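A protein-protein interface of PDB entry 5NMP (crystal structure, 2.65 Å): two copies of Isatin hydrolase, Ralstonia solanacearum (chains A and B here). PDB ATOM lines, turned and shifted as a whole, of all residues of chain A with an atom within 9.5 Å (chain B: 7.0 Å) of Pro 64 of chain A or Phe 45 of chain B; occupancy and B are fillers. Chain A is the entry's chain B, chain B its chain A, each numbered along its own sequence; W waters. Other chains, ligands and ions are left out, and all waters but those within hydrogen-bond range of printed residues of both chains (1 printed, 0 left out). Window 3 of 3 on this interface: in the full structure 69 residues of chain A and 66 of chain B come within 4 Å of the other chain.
Phe 45 of chain B touches two residues of chain A.
Gly 46 of chain B touches three residues of chain A.
Of the printed residues of chain B, Ala 65 of chain A touches Ile 88 (2.9 Å).
Printed residues of chain A within 4 Å of Gln 47 of chain B: Ile 56.
The nearest residue of chain A that does not touch Phe 45 of chain B is Ala 61 of chain A (4.1 Å).
The nearest printed residue of chain A that does not touch Leu 41 of chain B is Trp 66 of chain A (4.1 Å).
CG2 of Ile 56 of chain A touches C of Gly 46 of chain B, 3.4 Å away.
N of Gln 47 of chain B touches CG2 of Ile 56 of chain A, 3.7 Å away.
CA of Ile 88 of chain B touches CE1 of Tyr 59 of chain A, at 3.5 Å.
O of Ser 62 of chain A touches CB of Phe 45 of chain B (3.5 Å).
Pro 64 of chain A touches Phe 45 of chain B.
CD1 of Ile 88 of chain B touches O of Pro 64 of chain A (3.8 Å).
Trp 68 of chain A touches Leu 41 of chain B.
Gly 46 of chain B touches Trp 68 of chain A.
No position is printed for both chains.
The backbone NH (N) of Gly 46 of chain B lies within hydrogen-bond range of the backbone carbonyl oxygen (O) of Ser 62 of chain A.
The backbone NH (N) of Ile 88 of chain B sits at hydrogen-bond distance from the backbone carbonyl oxygen (O) of Ala 65 of chain A (2.9 Å).
OE1 of Gln 47 of chain B sits at hydrogen-bond distance from N of Leu 41 of chain B, 2.9 Å away.
The side-chain amide nitrogen (NE2) of Gln 47 of chain B sits at hydrogen-bond distance from the backbone carbonyl oxygen (O) of Pro 42 of chain B, at 3.2 Å.
NE2 of Gln 47 of chain B sits at hydrogen-bond distance from O of Phe 45 of chain B (3.1 Å).
The backbone NH (N) of Ile 56 of chain A sits at hydrogen-bond distance from the backbone carbonyl oxygen (O) of Trp 68 of chain A, at 2.9 Å.
OG of Ser 57 of chain A lies within hydrogen-bond range of NE1 of Trp 68 of chain A, at 3.3 Å.
O of Trp 66 of chain A lies within hydrogen-bond range of N of Tyr 59 of chain A.
Water W1 lies within hydrogen-bond range of O of Gly 46 of chain B (2.8 Å), O of Ser 62 of chain A (2.8 Å), NE1 of Trp 68 of chain A (3.0 Å) and NE1 of Trp 66 of chain A (3.0 Å).
Of the 13 printed residues of chain A, 6 touch a printed residue of chain B.
Hydrophobic or aromatic side chains of chain A within 4 Å of the printed part of chain B: Ile 56, Tyr 59, Pro 64 and Trp 68.
Of the 8 printed residues of chain B, 5 touch a printed residue of chain A.
Hydrophobic or aromatic side chains of chain B that line the printed part of chain A: Leu 41, Phe 45 and Ile 88.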
ATOM      1  N   ILE A  56       0.837   3.683  19.397  1.00  0.00           N
ATOM      2  CA  ILE A  56       1.061   2.893  20.597  1.00  0.00           C
ATOM      3  C   ILE A  56       2.306   2.037  20.398  1.00  0.00           C
ATOM      4  O   ILE A  56       3.172   1.961  21.270  1.00  0.00           O
ATOM      5  CB  ILE A  56      -0.147   1.998  20.921  1.00  0.00           C
ATOM      6  CG1 ILE A  56      -1.431   2.831  20.957  1.00  0.00           C
ATOM      7  CG2 ILE A  56       0.069   1.275  22.236  1.00  0.00           C
ATOM      8  CD1 ILE A  56      -2.689   2.011  21.106  1.00  0.00           C
ATOM      9  N   SER A  57       2.387   1.405  19.230  1.00  0.00           N
ATOM     10  CA  SER A  57       3.543   0.607  18.847  1.00  0.00           C
ATOM     11  C   SER A  57       3.602   0.483  17.326  1.00  0.00           C
ATOM     12  O   SER A  57       2.610   0.723  16.643  1.00  0.00           O
ATOM     13  CB  SER A  57       3.491  -0.778  19.497  1.00  0.00           C
ATOM     14  OG  SER A  57       2.434  -1.559  18.966  1.00  0.00           O
ATOM     15  N   HIS A  58       4.765   0.112  16.803  1.00  0.00           N
ATOM     16  CA  HIS A  58       4.954  -0.018  15.361  1.00  0.00           C
ATOM     17  C   HIS A  58       5.950  -1.136  15.061  1.00  0.00           C
ATOM     18  O   HIS A  58       7.054  -0.885  14.571  1.00  0.00           O
ATOM     19  CB  HIS A  58       5.430   1.311  14.762  1.00  0.00           C
ATOM     20  CG  HIS A  58       5.566   1.293  13.271  1.00  0.00           C
ATOM     21  ND1 HIS A  58       4.478   1.247  12.424  1.00  0.00           N
ATOM     22  CD2 HIS A  58       6.661   1.315  12.474  1.00  0.00           C
ATOM     23  CE1 HIS A  58       4.898   1.240  11.171  1.00  0.00           C
ATOM     24  NE2 HIS A  58       6.218   1.279  11.175  1.00  0.00           N
ATOM     25  N   TYR A  59       5.544  -2.367  15.361  1.00  0.00           N
ATOM     26  CA  TYR A  59       6.405  -3.543  15.233  1.00  0.00           C
ATOM     27  C   TYR A  59       7.752  -3.328  15.923  1.00  0.00           C
ATOM     28  O   TYR A  59       8.801  -3.636  15.361  1.00  0.00           O
ATOM     29  CB  TYR A  59       6.631  -3.898  13.762  1.00  0.00           C
ATOM     30  CG  TYR A  59       5.456  -3.621  12.847  1.00  0.00           C
ATOM     31  CD1 TYR A  59       4.297  -4.384  12.911  1.00  0.00           C
ATOM     32  CD2 TYR A  59       5.521  -2.609  11.899  1.00  0.00           C
ATOM     33  CE1 TYR A  59       3.230  -4.134  12.067  1.00  0.00           C
ATOM     34  CE2 TYR A  59       4.461  -2.351  11.052  1.00  0.00           C
ATOM     35  CZ  TYR A  59       3.318  -3.116  11.138  1.00  0.00           C
ATOM     36  OH  TYR A  59       2.264  -2.854  10.292  1.00  0.00           O
ATOM     37  N   ASP A  60       7.718  -2.792  17.138  1.00  0.00           N
ATOM     38  CA  ASP A  60       8.938  -2.464  17.867  1.00  0.00           C
ATOM     39  C   ASP A  60       8.876  -2.946  19.315  1.00  0.00           C
ATOM     40  O   ASP A  60       8.134  -3.870  19.634  1.00  0.00           O
ATOM     41  CB  ASP A  60       9.196  -0.955  17.818  1.00  0.00           C
ATOM     42  CG  ASP A  60       7.928  -0.136  17.999  1.00  0.00           C
ATOM     43  OD1 ASP A  60       7.002  -0.605  18.695  1.00  0.00           O
ATOM     44  OD2 ASP A  60       7.858   0.979  17.442  1.00  0.00           O
ATOM     45  N   ALA A  61       9.657  -2.318  20.189  1.00  0.00           N
ATOM     46  CA  ALA A  61       9.729  -2.731  21.588  1.00  0.00           C
ATOM     47  C   ALA A  61       8.382  -2.600  22.313  1.00  0.00           C
ATOM     48  O   ALA A  61       8.076  -3.387  23.209  1.00  0.00           O
ATOM     49  CB  ALA A  61      10.795  -1.930  22.313  1.00  0.00           C
ATOM     50  N   SER A  62       7.580  -1.614  21.919  1.00  0.00           N
ATOM     51  CA  SER A  62       6.274  -1.388  22.538  1.00  0.00           C
ATOM     52  C   SER A  62       5.221  -2.387  22.061  1.00  0.00           C
ATOM     53  O   SER A  62       4.137  -2.475  22.634  1.00  0.00           O
ATOM     54  CB  SER A  62       5.788   0.034  22.257  1.00  0.00           C
ATOM     55  OG  SER A  62       6.688   0.992  22.778  1.00  0.00           O
ATOM     56  N   GLY A  63       5.546  -3.129  21.007  1.00  0.00           N
ATOM     57  CA  GLY A  63       4.632  -4.102  20.432  1.00  0.00           C
ATOM     58  C   GLY A  63       5.285  -4.799  19.256  1.00  0.00           C
ATOM     59  O   GLY A  63       5.092  -4.395  18.110  1.00  0.00           O
ATOM     60  N   PRO A  64       6.072  -5.849  19.541  1.00  0.00           N
ATOM     61  CA  PRO A  64       6.947  -6.553  18.593  1.00  0.00           C
ATOM     62  C   PRO A  64       6.288  -6.998  17.289  1.00  0.00           C
ATOM     63  O   PRO A  64       6.930  -6.910  16.243  1.00  0.00           O
ATOM     64  CB  PRO A  64       7.406  -7.769  19.398  1.00  0.00           C
ATOM     65  CG  PRO A  64       7.410  -7.288  20.799  1.00  0.00           C
ATOM     66  CD  PRO A  64       6.210  -6.386  20.907  1.00  0.00           C
ATOM     67  N   ALA A  65       5.043  -7.462  17.337  1.00  0.00           N
ATOM     68  CA  ALA A  65       4.420  -8.040  16.150  1.00  0.00           C
ATOM     69  C   ALA A  65       3.185  -7.282  15.664  1.00  0.00           C
ATOM     70  O   ALA A  65       2.483  -7.756  14.769  1.00  0.00           O
ATOM     71  CB  ALA A  65       4.059  -9.500  16.413  1.00  0.00           C
ATOM     72  N   TRP A  66       2.919  -6.109  16.233  1.00  0.00           N
ATOM     73  CA  TRP A  66       1.716  -5.373  15.856  1.00  0.00           C
ATOM     74  C   TRP A  66       1.886  -3.858  15.827  1.00  0.00           C
ATOM     75  O   TRP A  66       2.840  -3.303  16.373  1.00  0.00           O
ATOM     76  CB  TRP A  66       0.558  -5.736  16.792  1.00  0.00           C
ATOM     77  CG  TRP A  66       0.852  -5.535  18.243  1.00  0.00           C
ATOM     78  CD1 TRP A  66       0.591  -4.422  18.988  1.00  0.00           C
ATOM     79  CD2 TRP A  66       1.460  -6.479  19.133  1.00  0.00           C
ATOM     80  NE1 TRP A  66       1.000  -4.614  20.287  1.00  0.00           N
ATOM     81  CE2 TRP A  66       1.537  -5.869  20.401  1.00  0.00           C
ATOM     82  CE3 TRP A  66       1.947  -7.781  18.980  1.00  0.00           C
ATOM     83  CZ2 TRP A  66       2.083  -6.516  21.508  1.00  0.00           C
ATOM     84  CZ3 TRP A  66       2.488  -8.420  20.080  1.00  0.00           C
ATOM     85  CH2 TRP A  66       2.552  -7.787  21.326  1.00  0.00           C
ATOM     86  N   TYR A  67       0.931  -3.203  15.175  1.00  0.00           N
ATOM     87  CA  TYR A  67       0.906  -1.755  15.044  1.00  0.00           C
ATOM     88  C   TYR A  67      -0.512  -1.243  15.299  1.00  0.00           C
ATOM     89  O   TYR A  67      -1.477  -1.807  14.784  1.00  0.00           O
ATOM     90  CB  TYR A  67       1.404  -1.350  13.653  1.00  0.00           C
ATOM     91  CG  TYR A  67       0.866  -0.037  13.122  1.00  0.00           C
ATOM     92  CD1 TYR A  67       1.266   1.175  13.667  1.00  0.00           C
ATOM     93  CD2 TYR A  67      -0.021  -0.014  12.053  1.00  0.00           C
ATOM     94  CE1 TYR A  67       0.781   2.374  13.175  1.00  0.00           C
ATOM     95  CE2 TYR A  67      -0.508   1.177  11.553  1.00  0.00           C
ATOM     96  CZ  TYR A  67      -0.105   2.369  12.116  1.00  0.00           C
ATOM     97  OH  TYR A  67      -0.594   3.556  11.618  1.00  0.00           O
ATOM     98  N   TRP A  68      -0.638  -0.197  16.112  1.00  0.00           N
ATOM     99  CA  TRP A  68      -1.949   0.382  16.413  1.00  0.00           C
ATOM    100  C   TRP A  68      -1.839   1.770  17.051  1.00  0.00           C
ATOM    101  O   TRP A  68      -0.793   2.138  17.593  1.00  0.00           O
ATOM    102  CB  TRP A  68      -2.773  -0.554  17.318  1.00  0.00           C
ATOM    103  CG  TRP A  68      -2.132  -0.959  18.625  1.00  0.00           C
ATOM    104  CD1 TRP A  68      -0.823  -0.813  18.989  1.00  0.00           C
ATOM    105  CD2 TRP A  68      -2.786  -1.581  19.739  1.00  0.00           C
ATOM    106  NE1 TRP A  68      -0.623  -1.303  20.258  1.00  0.00           N
ATOM    107  CE2 TRP A  68      -1.813  -1.779  20.740  1.00  0.00           C
ATOM    108  CE3 TRP A  68      -4.101  -1.987  19.988  1.00  0.00           C
ATOM    109  CZ2 TRP A  68      -2.115  -2.365  21.969  1.00  0.00           C
ATOM    110  CZ3 TRP A  68      -4.397  -2.567  21.209  1.00  0.00           C
ATOM    111  CH2 TRP A  68      -3.409  -2.751  22.184  1.00  0.00           C
ATOM    112  N   LEU B  41      -2.542  -5.225  28.149  1.00  0.00           N
ATOM    113  CA  LEU B  41      -1.397  -6.073  27.841  1.00  0.00           C
ATOM    114  C   LEU B  41      -0.410  -6.039  29.000  1.00  0.00           C
ATOM    115  O   LEU B  41      -0.513  -5.166  29.865  1.00  0.00           O
ATOM    116  CB  LEU B  41      -0.718  -5.604  26.552  1.00  0.00           C
ATOM    117  CG  LEU B  41      -1.592  -5.429  25.315  1.00  0.00           C
ATOM    118  CD1 LEU B  41      -0.728  -5.059  24.124  1.00  0.00           C
ATOM    119  CD2 LEU B  41      -2.385  -6.691  25.039  1.00  0.00           C
ATOM    120  N   PRO B  42       0.544  -6.989  29.032  1.00  0.00           N
ATOM    121  CA  PRO B  42       1.639  -6.932  30.008  1.00  0.00           C
ATOM    122  C   PRO B  42       2.317  -5.561  30.045  1.00  0.00           C
ATOM    123  O   PRO B  42       2.382  -4.881  29.018  1.00  0.00           O
ATOM    124  CB  PRO B  42       2.601  -8.008  29.507  1.00  0.00           C
ATOM    125  CG  PRO B  42       1.706  -9.016  28.880  1.00  0.00           C
ATOM    126  CD  PRO B  42       0.570  -8.245  28.260  1.00  0.00           C
ATOM    127  N   SER B  43       2.816  -5.174  31.215  1.00  0.00           N
ATOM    128  CA  SER B  43       3.273  -3.807  31.462  1.00  0.00           C
ATOM    129  C   SER B  43       4.404  -3.342  30.543  1.00  0.00           C
ATOM    130  O   SER B  43       4.627  -2.140  30.389  1.00  0.00           O
ATOM    131  CB  SER B  43       3.717  -3.667  32.918  1.00  0.00           C
ATOM    132  OG  SER B  43       4.784  -4.550  33.211  1.00  0.00           O
ATOM    133  N   GLN B  44       5.111  -4.288  29.933  1.00  0.00           N
ATOM    134  CA  GLN B  44       6.238  -3.955  29.070  1.00  0.00           C
ATOM    135  C   GLN B  44       5.794  -3.402  27.716  1.00  0.00           C
ATOM    136  O   GLN B  44       6.604  -2.868  26.965  1.00  0.00           O
ATOM    137  CB  GLN B  44       7.123  -5.181  28.858  1.00  0.00           C
ATOM    138  CG  GLN B  44       6.472  -6.273  28.026  1.00  0.00           C
ATOM    139  CD  GLN B  44       6.423  -7.605  28.745  1.00  0.00           C
ATOM    140  OE1 GLN B  44       5.976  -7.689  29.891  1.00  0.00           O
ATOM    141  NE2 GLN B  44       6.890  -8.656  28.077  1.00  0.00           N
ATOM    142  N   PHE B  45       4.508  -3.531  27.407  1.00  0.00           N
ATOM    143  CA  PHE B  45       3.984  -3.070  26.125  1.00  0.00           C
ATOM    144  C   PHE B  45       3.200  -1.762  26.242  1.00  0.00           C
ATOM    145  O   PHE B  45       2.779  -1.369  27.330  1.00  0.00           O
ATOM    146  CB  PHE B  45       3.088  -4.140  25.496  1.00  0.00           C
ATOM    147  CG  PHE B  45       3.755  -5.473  25.329  1.00  0.00           C
ATOM    148  CD1 PHE B  45       4.916  -5.595  24.587  1.00  0.00           C
ATOM    149  CD2 PHE B  45       3.210  -6.610  25.900  1.00  0.00           C
ATOM    150  CE1 PHE B  45       5.528  -6.826  24.427  1.00  0.00           C
ATOM    151  CE2 PHE B  45       3.817  -7.844  25.742  1.00  0.00           C
ATOM    152  CZ  PHE B  45       4.975  -7.949  25.004  1.00  0.00           C
ATOM    153  N   GLY B  46       3.009  -1.095  25.108  1.00  0.00           N
ATOM    154  CA  GLY B  46       2.163   0.082  25.045  1.00  0.00           C
ATOM    155  C   GLY B  46       0.703  -0.309  25.178  1.00  0.00           C
ATOM    156  O   GLY B  46       0.287  -1.357  24.682  1.00  0.00           O
ATOM    157  N   GLN B  47      -0.080   0.536  25.838  1.00  0.00           N
ATOM    158  CA  GLN B  47      -1.470   0.211  26.145  1.00  0.00           C
ATOM    159  C   GLN B  47      -2.458   1.043  25.335  1.00  0.00           C
ATOM    160  O   GLN B  47      -2.192   2.199  25.012  1.00  0.00           O
ATOM    161  CB  GLN B  47      -1.737   0.408  27.640  1.00  0.00           C
ATOM    162  CG  GLN B  47      -0.745  -0.294  28.551  1.00  0.00           C
ATOM    163  CD  GLN B  47      -0.860  -1.803  28.490  1.00  0.00           C
ATOM    164  OE1 GLN B  47      -1.936  -2.348  28.250  1.00  0.00           O
ATOM    165  NE2 GLN B  47       0.255  -2.490  28.708  1.00  0.00           N
ATOM    166  N   ILE B  88       2.386  -7.636  11.848  1.00  0.00           N
ATOM    167  CA  ILE B  88       3.668  -7.512  11.160  1.00  0.00           C
ATOM    168  C   ILE B  88       3.720  -8.293   9.841  1.00  0.00           C
ATOM    169  O   ILE B  88       4.494  -7.954   8.945  1.00  0.00           O
ATOM    170  CB  ILE B  88       4.830  -7.970  12.085  1.00  0.00           C
ATOM    171  CG1 ILE B  88       6.175  -7.449  11.575  1.00  0.00           C
ATOM    172  CG2 ILE B  88       4.839  -9.482  12.254  1.00  0.00           C
ATOM    173  CD1 ILE B  88       7.309  -7.660  12.547  1.00  0.00           C
HETATM  174  O   HOH W   1       1.338  -2.318  22.239  1.00  0.00           O
